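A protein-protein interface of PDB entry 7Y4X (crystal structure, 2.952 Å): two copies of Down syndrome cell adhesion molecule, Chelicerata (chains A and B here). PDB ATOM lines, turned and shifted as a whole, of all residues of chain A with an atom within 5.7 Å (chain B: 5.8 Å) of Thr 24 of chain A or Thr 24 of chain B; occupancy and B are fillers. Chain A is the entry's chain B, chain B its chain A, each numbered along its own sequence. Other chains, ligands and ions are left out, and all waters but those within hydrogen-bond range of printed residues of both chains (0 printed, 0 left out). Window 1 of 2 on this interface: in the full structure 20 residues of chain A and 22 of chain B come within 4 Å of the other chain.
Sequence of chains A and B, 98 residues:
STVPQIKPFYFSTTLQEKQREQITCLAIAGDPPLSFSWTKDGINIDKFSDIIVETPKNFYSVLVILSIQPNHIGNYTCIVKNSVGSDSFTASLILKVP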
ATOM      1  N   LYS A   7      15.202 -18.163   0.848  1.00  0.00           N
ATOM      2  CA  LYS A   7      16.613 -18.288   0.525  1.00  0.00           C
ATOM      3  C   LYS A   7      17.338 -18.941   1.696  1.00  0.00           C
ATOM      4  O   LYS A   7      17.114 -18.552   2.848  1.00  0.00           O
ATOM      5  CB  LYS A   7      17.207 -16.918   0.219  1.00  0.00           C
ATOM      6  CG  LYS A   7      18.688 -16.920  -0.091  1.00  0.00           C
ATOM      7  CD  LYS A   7      19.137 -15.545  -0.560  1.00  0.00           C
ATOM      8  CE  LYS A   7      20.629 -15.360  -0.366  1.00  0.00           C
ATOM      9  NZ  LYS A   7      21.010 -13.931  -0.529  1.00  0.00           N
ATOM     10  N   PRO A   8      18.186 -19.939   1.452  1.00  0.00           N
ATOM     11  CA  PRO A   8      18.911 -20.580   2.557  1.00  0.00           C
ATOM     12  C   PRO A   8      19.779 -19.578   3.299  1.00  0.00           C
ATOM     13  O   PRO A   8      20.392 -18.694   2.697  1.00  0.00           O
ATOM     14  CB  PRO A   8      19.757 -21.647   1.851  1.00  0.00           C
ATOM     15  CG  PRO A   8      19.038 -21.918   0.570  1.00  0.00           C
ATOM     16  CD  PRO A   8      18.430 -20.607   0.163  1.00  0.00           C
ATOM     17  N   PHE A   9      19.811 -19.712   4.623  1.00  0.00           N
ATOM     18  CA  PHE A   9      20.641 -18.874   5.473  1.00  0.00           C
ATOM     19  C   PHE A   9      21.469 -19.758   6.394  1.00  0.00           C
ATOM     20  O   PHE A   9      21.110 -20.902   6.684  1.00  0.00           O
ATOM     21  CB  PHE A   9      19.803 -17.878   6.292  1.00  0.00           C
ATOM     22  CG  PHE A   9      18.641 -18.500   7.012  1.00  0.00           C
ATOM     23  CD1 PHE A   9      18.805 -19.053   8.273  1.00  0.00           C
ATOM     24  CD2 PHE A   9      17.382 -18.520   6.435  1.00  0.00           C
ATOM     25  CE1 PHE A   9      17.736 -19.621   8.940  1.00  0.00           C
ATOM     26  CE2 PHE A   9      16.308 -19.088   7.099  1.00  0.00           C
ATOM     27  CZ  PHE A   9      16.485 -19.638   8.352  1.00  0.00           C
ATOM     28  N   GLN A  22      23.949 -12.542  12.563  1.00  0.00           N
ATOM     29  CA  GLN A  22      22.730 -12.129  11.882  1.00  0.00           C
ATOM     30  C   GLN A  22      22.385 -13.162  10.821  1.00  0.00           C
ATOM     31  O   GLN A  22      23.264 -13.612  10.082  1.00  0.00           O
ATOM     32  CB  GLN A  22      22.890 -10.746  11.240  1.00  0.00           C
ATOM     33  CG  GLN A  22      21.580 -10.143  10.751  1.00  0.00           C
ATOM     34  CD  GLN A  22      21.390 -10.276   9.248  1.00  0.00           C
ATOM     35  OE1 GLN A  22      21.760 -11.286   8.647  1.00  0.00           O
ATOM     36  NE2 GLN A  22      20.792  -9.261   8.637  1.00  0.00           N
ATOM     37  N   ILE A  23      21.109 -13.533  10.754  1.00  0.00           N
ATOM     38  CA  ILE A  23      20.579 -14.337   9.661  1.00  0.00           C
ATOM     39  C   ILE A  23      19.296 -13.680   9.178  1.00  0.00           C
ATOM     40  O   ILE A  23      18.559 -13.066   9.957  1.00  0.00           O
ATOM     41  CB  ILE A  23      20.317 -15.805  10.070  1.00  0.00           C
ATOM     42  CG1 ILE A  23      19.485 -15.868  11.352  1.00  0.00           C
ATOM     43  CG2 ILE A  23      21.626 -16.559  10.235  1.00  0.00           C
ATOM     44  CD1 ILE A  23      18.883 -17.227  11.617  1.00  0.00           C
ATOM     45  N   THR A  24      19.033 -13.801   7.879  1.00  0.00           N
ATOM     46  CA  THR A  24      17.861 -13.198   7.261  1.00  0.00           C
ATOM     47  C   THR A  24      17.029 -14.286   6.604  1.00  0.00           C
ATOM     48  O   THR A  24      17.520 -15.015   5.733  1.00  0.00           O
ATOM     49  CB  THR A  24      18.248 -12.132   6.237  1.00  0.00           C
ATOM     50  OG1 THR A  24      18.972 -11.086   6.894  1.00  0.00           O
ATOM     51  CG2 THR A  24      17.004 -11.555   5.562  1.00  0.00           C
ATOM     52  N   CYS A  25      15.772 -14.391   7.028  1.00  0.00           N
ATOM     53  CA  CYS A  25      14.789 -15.249   6.370  1.00  0.00           C
ATOM     54  C   CYS A  25      14.187 -14.459   5.216  1.00  0.00           C
ATOM     55  O   CYS A  25      13.203 -13.734   5.375  1.00  0.00           O
ATOM     56  CB  CYS A  25      13.723 -15.698   7.356  1.00  0.00           C
ATOM     57  SG  CYS A  25      12.644 -17.023   6.816  1.00  0.00           S
ATOM     58  N   LEU A  26      14.799 -14.578   4.042  1.00  0.00           N
ATOM     59  CA  LEU A  26      14.389 -13.816   2.872  1.00  0.00           C
ATOM     60  C   LEU A  26      13.415 -14.630   2.030  1.00  0.00           C
ATOM     61  O   LEU A  26      13.691 -15.785   1.691  1.00  0.00           O
ATOM     62  CB  LEU A  26      15.599 -13.412   2.027  1.00  0.00           C
ATOM     63  CG  LEU A  26      15.281 -12.867   0.629  1.00  0.00           C
ATOM     64  CD1 LEU A  26      14.584 -11.517   0.712  1.00  0.00           C
ATOM     65  CD2 LEU A  26      16.530 -12.772  -0.237  1.00  0.00           C
ATOM     66  N   TRP A  38       9.502 -17.431  13.911  1.00  0.00           N
ATOM     67  CA  TRP A  38      10.771 -18.039  14.283  1.00  0.00           C
ATOM     68  C   TRP A  38      10.605 -18.952  15.488  1.00  0.00           C
ATOM     69  O   TRP A  38       9.851 -18.643  16.416  1.00  0.00           O
ATOM     70  CB  TRP A  38      11.829 -16.980  14.608  1.00  0.00           C
ATOM     71  CG  TRP A  38      12.299 -16.204  13.425  1.00  0.00           C
ATOM     72  CD1 TRP A  38      11.738 -15.072  12.914  1.00  0.00           C
ATOM     73  CD2 TRP A  38      13.433 -16.499  12.603  1.00  0.00           C
ATOM     74  NE1 TRP A  38      12.452 -14.643  11.822  1.00  0.00           N
ATOM     75  CE2 TRP A  38      13.498 -15.502  11.610  1.00  0.00           C
ATOM     76  CE3 TRP A  38      14.400 -17.509  12.608  1.00  0.00           C
ATOM     77  CZ2 TRP A  38      14.491 -15.484  10.636  1.00  0.00           C
ATOM     78  CZ3 TRP A  38      15.383 -17.492  11.637  1.00  0.00           C
ATOM     79  CH2 TRP A  38      15.421 -16.486  10.664  1.00  0.00           C
ATOM     80  N   TYR A  60      11.078  -9.914   4.052  1.00  0.00           N
ATOM     81  CA  TYR A  60      12.093 -10.645   4.799  1.00  0.00           C
ATOM     82  C   TYR A  60      12.000 -10.275   6.272  1.00  0.00           C
ATOM     83  O   TYR A  60      11.442  -9.237   6.639  1.00  0.00           O
ATOM     84  CB  TYR A  60      13.511 -10.398   4.255  1.00  0.00           C
ATOM     85  CG  TYR A  60      14.084  -9.001   4.426  1.00  0.00           C
ATOM     86  CD1 TYR A  60      14.661  -8.603   5.626  1.00  0.00           C
ATOM     87  CD2 TYR A  60      14.093  -8.100   3.368  1.00  0.00           C
ATOM     88  CE1 TYR A  60      15.201  -7.336   5.779  1.00  0.00           C
ATOM     89  CE2 TYR A  60      14.632  -6.832   3.512  1.00  0.00           C
ATOM     90  CZ  TYR A  60      15.185  -6.456   4.718  1.00  0.00           C
ATOM     91  OH  TYR A  60      15.721  -5.198   4.865  1.00  0.00           O
ATOM     92  N   SER A  61      12.544 -11.156   7.111  1.00  0.00           N
ATOM     93  CA  SER A  61      12.630 -10.949   8.549  1.00  0.00           C
ATOM     94  C   SER A  61      14.041 -11.287   9.002  1.00  0.00           C
ATOM     95  O   SER A  61      14.671 -12.202   8.465  1.00  0.00           O
ATOM     96  CB  SER A  61      11.608 -11.809   9.306  1.00  0.00           C
ATOM     97  OG  SER A  61      11.902 -11.848  10.691  1.00  0.00           O
ATOM     98  N   VAL A  62      14.533 -10.550   9.995  1.00  0.00           N
ATOM     99  CA  VAL A  62      15.930 -10.615  10.407  1.00  0.00           C
ATOM    100  C   VAL A  62      16.009 -11.054  11.863  1.00  0.00           C
ATOM    101  O   VAL A  62      15.198 -10.634  12.696  1.00  0.00           O
ATOM    102  CB  VAL A  62      16.632  -9.255  10.201  1.00  0.00           C
ATOM    103  CG1 VAL A  62      18.080  -9.326  10.643  1.00  0.00           C
ATOM    104  CG2 VAL A  62      16.537  -8.828   8.744  1.00  0.00           C
ATOM    105  N   LEU A  63      16.988 -11.908  12.161  1.00  0.00           N
ATOM    106  CA  LEU A  63      17.279 -12.365  13.513  1.00  0.00           C
ATOM    107  C   LEU A  63      18.712 -11.979  13.851  1.00  0.00           C
ATOM    108  O   LEU A  63      19.638 -12.311  13.104  1.00  0.00           O
ATOM    109  CB  LEU A  63      17.081 -13.880  13.631  1.00  0.00           C
ATOM    110  CG  LEU A  63      17.149 -14.525  15.017  1.00  0.00           C
ATOM    111  CD1 LEU A  63      16.122 -15.638  15.134  1.00  0.00           C
ATOM    112  CD2 LEU A  63      18.546 -15.056  15.311  1.00  0.00           C
ATOM    113  N   LYS B   7      31.223 -11.502   7.895  1.00  0.00           N
ATOM    114  CA  LYS B   7      30.650 -12.827   7.707  1.00  0.00           C
ATOM    115  C   LYS B   7      30.236 -12.992   6.248  1.00  0.00           C
ATOM    116  O   LYS B   7      29.555 -12.116   5.703  1.00  0.00           O
ATOM    117  CB  LYS B   7      29.452 -13.035   8.625  1.00  0.00           C
ATOM    118  CG  LYS B   7      28.724 -14.348   8.401  1.00  0.00           C
ATOM    119  CD  LYS B   7      27.426 -14.390   9.182  1.00  0.00           C
ATOM    120  CE  LYS B   7      26.521 -15.502   8.682  1.00  0.00           C
ATOM    121  NZ  LYS B   7      25.132 -15.349   9.199  1.00  0.00           N
ATOM    122  N   PRO B   8      30.635 -14.079   5.589  1.00  0.00           N
ATOM    123  CA  PRO B   8      30.357 -14.226   4.155  1.00  0.00           C
ATOM    124  C   PRO B   8      28.868 -14.141   3.837  1.00  0.00           C
ATOM    125  O   PRO B   8      28.015 -14.550   4.629  1.00  0.00           O
ATOM    126  CB  PRO B   8      30.918 -15.614   3.829  1.00  0.00           C
ATOM    127  CG  PRO B   8      31.995 -15.823   4.838  1.00  0.00           C
ATOM    128  CD  PRO B   8      31.538 -15.128   6.093  1.00  0.00           C
ATOM    129  N   PHE B   9      28.569 -13.593   2.660  1.00  0.00           N
ATOM    130  CA  PHE B   9      27.210 -13.504   2.146  1.00  0.00           C
ATOM    131  C   PHE B   9      27.193 -13.980   0.698  1.00  0.00           C
ATOM    132  O   PHE B   9      28.205 -13.926  -0.005  1.00  0.00           O
ATOM    133  CB  PHE B   9      26.654 -12.075   2.245  1.00  0.00           C
ATOM    134  CG  PHE B   9      27.581 -11.019   1.709  1.00  0.00           C
ATOM    135  CD1 PHE B   9      27.589 -10.703   0.360  1.00  0.00           C
ATOM    136  CD2 PHE B   9      28.437 -10.335   2.556  1.00  0.00           C
ATOM    137  CE1 PHE B   9      28.439  -9.731  -0.136  1.00  0.00           C
ATOM    138  CE2 PHE B   9      29.289  -9.360   2.068  1.00  0.00           C
ATOM    139  CZ  PHE B   9      29.289  -9.058   0.721  1.00  0.00           C
ATOM    140  N   GLN B  22      18.340 -10.102  -1.145  1.00  0.00           N
ATOM    141  CA  GLN B  22      18.909  -9.357  -0.034  1.00  0.00           C
ATOM    142  C   GLN B  22      20.204 -10.031   0.389  1.00  0.00           C
ATOM    143  O   GLN B  22      20.277 -11.261   0.461  1.00  0.00           O
ATOM    144  CB  GLN B  22      17.946  -9.277   1.156  1.00  0.00           C
ATOM    145  CG  GLN B  22      18.359  -8.277   2.234  1.00  0.00           C
ATOM    146  CD  GLN B  22      19.022  -8.926   3.440  1.00  0.00           C
ATOM    147  OE1 GLN B  22      19.975  -9.693   3.306  1.00  0.00           O
ATOM    148  NE2 GLN B  22      18.520  -8.613   4.629  1.00  0.00           N
ATOM    149  N   ILE B  23      21.224  -9.219   0.653  1.00  0.00           N
ATOM    150  CA  ILE B  23      22.457  -9.691   1.266  1.00  0.00           C
ATOM    151  C   ILE B  23      22.822  -8.741   2.394  1.00  0.00           C
ATOM    152  O   ILE B  23      22.584  -7.530   2.319  1.00  0.00           O
ATOM    153  CB  ILE B  23      23.622  -9.813   0.260  1.00  0.00           C
ATOM    154  CG1 ILE B  23      23.716  -8.560  -0.607  1.00  0.00           C
ATOM    155  CG2 ILE B  23      23.463 -11.064  -0.590  1.00  0.00           C
ATOM    156  CD1 ILE B  23      25.054  -8.397  -1.283  1.00  0.00           C
ATOM    157  N   THR B  24      23.389  -9.306   3.456  1.00  0.00           N
ATOM    158  CA  THR B  24      23.780  -8.552   4.638  1.00  0.00           C
ATOM    159  C   THR B  24      25.281  -8.686   4.829  1.00  0.00           C
ATOM    160  O   THR B  24      25.806  -9.802   4.912  1.00  0.00           O
ATOM    161  CB  THR B  24      23.043  -9.039   5.886  1.00  0.00           C
ATOM    162  OG1 THR B  24      21.637  -8.858   5.705  1.00  0.00           O
ATOM    163  CG2 THR B  24      23.501  -8.244   7.107  1.00  0.00           C
ATOM    164  N   CYS B  25      25.966  -7.547   4.892  1.00  0.00           N
ATOM    165  CA  CYS B  25      27.392  -7.495   5.205  1.00  0.00           C
ATOM    166  C   CYS B  25      27.525  -7.310   6.707  1.00  0.00           C
ATOM    167  O   CYS B  25      27.526  -6.192   7.218  1.00  0.00           O
ATOM    168  CB  CYS B  25      28.074  -6.369   4.443  1.00  0.00           C
ATOM    169  SG  CYS B  25      29.862  -6.257   4.694  1.00  0.00           S
ATOM    170  N   LEU B  26      27.627  -8.421   7.429  1.00  0.00           N
ATOM    171  CA  LEU B  26      27.662  -8.383   8.886  1.00  0.00           C
ATOM    172  C   LEU B  26      29.103  -8.316   9.380  1.00  0.00           C
ATOM    173  O   LEU B  26      29.932  -9.154   9.013  1.00  0.00           O
ATOM    174  CB  LEU B  26      26.960  -9.606   9.471  1.00  0.00           C
ATOM    175  CG  LEU B  26      27.251  -9.894  10.951  1.00  0.00           C
ATOM    176  CD1 LEU B  26      26.542  -8.914  11.880  1.00  0.00           C
ATOM    177  CD2 LEU B  26      26.892 -11.324  11.300  1.00  0.00           C
ATOM    178  N   TRP B  38      29.793   0.039  -0.292  1.00  0.00           N
ATOM    179  CA  TRP B  38      29.485  -0.960  -1.302  1.00  0.00           C
ATOM    180  C   TRP B  38      29.943  -0.490  -2.673  1.00  0.00           C
ATOM    181  O   TRP B  38      29.889   0.702  -2.992  1.00  0.00           O
ATOM    182  CB  TRP B  38      27.982  -1.271  -1.363  1.00  0.00           C
ATOM    183  CG  TRP B  38      27.448  -1.975  -0.159  1.00  0.00           C
ATOM    184  CD1 TRP B  38      27.003  -1.400   0.993  1.00  0.00           C
ATOM    185  CD2 TRP B  38      27.289  -3.388   0.009  1.00  0.00           C
ATOM    186  NE1 TRP B  38      26.579  -2.366   1.871  1.00  0.00           N
ATOM    187  CE2 TRP B  38      26.744  -3.596   1.291  1.00  0.00           C
ATOM    188  CE3 TRP B  38      27.555  -4.499  -0.799  1.00  0.00           C
ATOM    189  CZ2 TRP B  38      26.460  -4.866   1.784  1.00  0.00           C
ATOM    190  CZ3 TRP B  38      27.273  -5.760  -0.306  1.00  0.00           C
ATOM    191  CH2 TRP B  38      26.732  -5.933   0.973  1.00  0.00           C
ATOM    192  N   TYR B  60      25.997  -3.904  10.831  1.00  0.00           N
ATOM    193  CA  TYR B  60      25.806  -4.606   9.570  1.00  0.00           C
ATOM    194  C   TYR B  60      25.098  -3.691   8.583  1.00  0.00           C
ATOM    195  O   TYR B  60      24.328  -2.807   8.969  1.00  0.00           O
ATOM    196  CB  TYR B  60      25.040  -5.930   9.738  1.00  0.00           C
ATOM    197  CG  TYR B  60      23.585  -5.838  10.163  1.00  0.00           C
ATOM    198  CD1 TYR B  60      22.577  -5.615   9.231  1.00  0.00           C
ATOM    199  CD2 TYR B  60      23.215  -6.035  11.487  1.00  0.00           C
ATOM    200  CE1 TYR B  60      21.247  -5.553   9.612  1.00  0.00           C
ATOM    201  CE2 TYR B  60      21.888  -5.977  11.878  1.00  0.00           C
ATOM    202  CZ  TYR B  60      20.909  -5.735  10.937  1.00  0.00           C
ATOM    203  OH  TYR B  60      19.589  -5.678  11.323  1.00  0.00           O
ATOM    204  N   SER B  61      25.388  -3.907   7.303  1.00  0.00           N
ATOM    205  CA  SER B  61      24.765  -3.181   6.208  1.00  0.00           C
ATOM    206  C   SER B  61      23.991  -4.155   5.331  1.00  0.00           C
ATOM    207  O   SER B  61      24.336  -5.336   5.233  1.00  0.00           O
ATOM    208  CB  SER B  61      25.807  -2.435   5.371  1.00  0.00           C
ATOM    209  OG  SER B  61      25.253  -1.984   4.149  1.00  0.00           O
ATOM    210  N   VAL B  62      22.938  -3.651   4.693  1.00  0.00           N
ATOM    211  CA  VAL B  62      21.989  -4.480   3.959  1.00  0.00           C
ATOM    212  C   VAL B  62      21.843  -3.929   2.548  1.00  0.00           C
ATOM    213  O   VAL B  62      21.672  -2.718   2.364  1.00  0.00           O
ATOM    214  CB  VAL B  62      20.620  -4.535   4.662  1.00  0.00           C
ATOM    215  CG1 VAL B  62      19.630  -5.333   3.837  1.00  0.00           C
ATOM    216  CG2 VAL B  62      20.762  -5.139   6.043  1.00  0.00           C
ATOM    217  N   LEU B  63      21.907  -4.817   1.558  1.00  0.00           N
ATOM    218  CA  LEU B  63      21.718  -4.475   0.153  1.00  0.00           C
ATOM    219  C   LEU B  63      20.498  -5.227  -0.358  1.00  0.00           C
ATOM    220  O   LEU B  63      20.441  -6.457  -0.258  1.00  0.00           O
ATOM    221  CB  LEU B  63      22.962  -4.829  -0.664  1.00  0.00           C
ATOM    222  CG  LEU B  63      23.066  -4.253  -2.075  1.00  0.00           C
ATOM    223  CD1 LEU B  63      24.381  -3.512  -2.261  1.00  0.00           C
ATOM    224  CD2 LEU B  63      22.921  -5.359  -3.105  1.00  0.00           C
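The side-chain hydroxyl (OG1) of Thr 24 of chain B is in hydrogen-bond range of the side-chain amide nitrogen (NE2) of Gln 22 of chain A, 3.1 Å away. NZ of Lys 7 of chain B sits at hydrogen-bond distance from O of Gln 22 of chain A (2.7 Å). The backbone carbonyl oxygen (O) of Gln 22 of chain B lies within hydrogen-bond range of the side-chain amino group (NZ) of Lys 7 of chain A (2.9 Å). OG1 of Thr 24 of chain A sits at hydrogen-bond distance from NE2 of Gln 22 of chain B, at 3.4 Å.
O of Ile 23 of chain B lies within hydrogen-bond range of N of Leu 63 of chain B (2.9 Å). The side-chain amide nitrogen (NE2) of Gln 22 of chain A is in hydrogen-bond range of the side-chain hydroxyl (OG1) of Thr 24 of chain A. OE1 of Gln 22 of chain B lies within hydrogen-bond range of OG1 of Thr 24 of chain B, 3.0 Å away. The backbone NH of Lys 7 of chain B is in hydrogen-bond range of the backbone carbonyl oxygen of Leu 26 of chain B. O of Ile 23 of chain A sits at hydrogen-bond distance from N of Leu 63 of chain A (2.9 Å). The backbone NH of Lys 7 of chain A is in hydrogen-bond range of the backbone carbonyl oxygen of Leu 26 of chain A (2.9 Å).
CG2 of Ile 23 of chain B touches NZ of Lys 7 of chain A, 3.8 Å away. N of Gln 22 of chain A touches CD2 of Leu 26 of chain B, 3.4 Å away. Tyr 60 of chain B touches Gln 22 of chain A (CE1 to NE2, 3.9 Å). CG2 of Ile 23 of chain A touches NZ of Lys 7 of chain B, at 3.9 Å. Thr 24 of chain B touches Thr 24 of chain A (OG1 to OG1, 3.7 Å). Leu 26 of chain A touches Gln 22 of chain B (CD2 to N, 3.4 Å). Tyr 60 of chain A touches Gln 22 of chain B.
Printed residues of chain B within 4 Å of Lys 7 of chain A: Gln 22 (2.9 Å) and Ile 23 (3.8 Å). Thr 24 of chain A touches just these residues of chain B: Gln 22 (3.4 Å) and Thr 24 (3.7 Å). Printed residues of chain A within 4 Å of Gln 22 of chain B: Lys 7 (2.9 Å), Thr 24 (3.4 Å), Leu 26 (3.4 Å) and Tyr 60 (3.7 Å). Printed residues of chain A within 4 Å of Thr 24 of chain B: Gln 22 and Thr 24. The nearest printed residue of chain B that does not touch Thr 24 of chain A is Val 62 of chain B (6.3 Å). The nearest printed residue of chain A that does not touch Lys 7 of chain B is Phe 9 of chain A (6.4 Å).
Of the 13 printed residues of chain A, 6 touch a printed residue of chain B. Hydrophobic or aromatic side chains of chain A that line the printed part of chain B: Ile 23, Leu 26 and Tyr 60. Among the printed residues, 11 pairs touch across the chains.
Lys 7 of chain A touches Gln 22 of chain B, and with the chains exchanged Gln 22 of chain A touches Lys 7 of chain B. Gln 22 of chain A touches Thr 24 of chain B, and with the chains exchanged Thr 24 of chain A touches Gln 22 of chain B. Gln 22 of chain A touches Tyr 60 of chain B, and with the chains exchanged Tyr 60 of chain A touches Gln 22 of chain B. Thr 24 of chain A touches its own counterpart, Thr 24 of chain B. 13 positions are printed for both chains.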
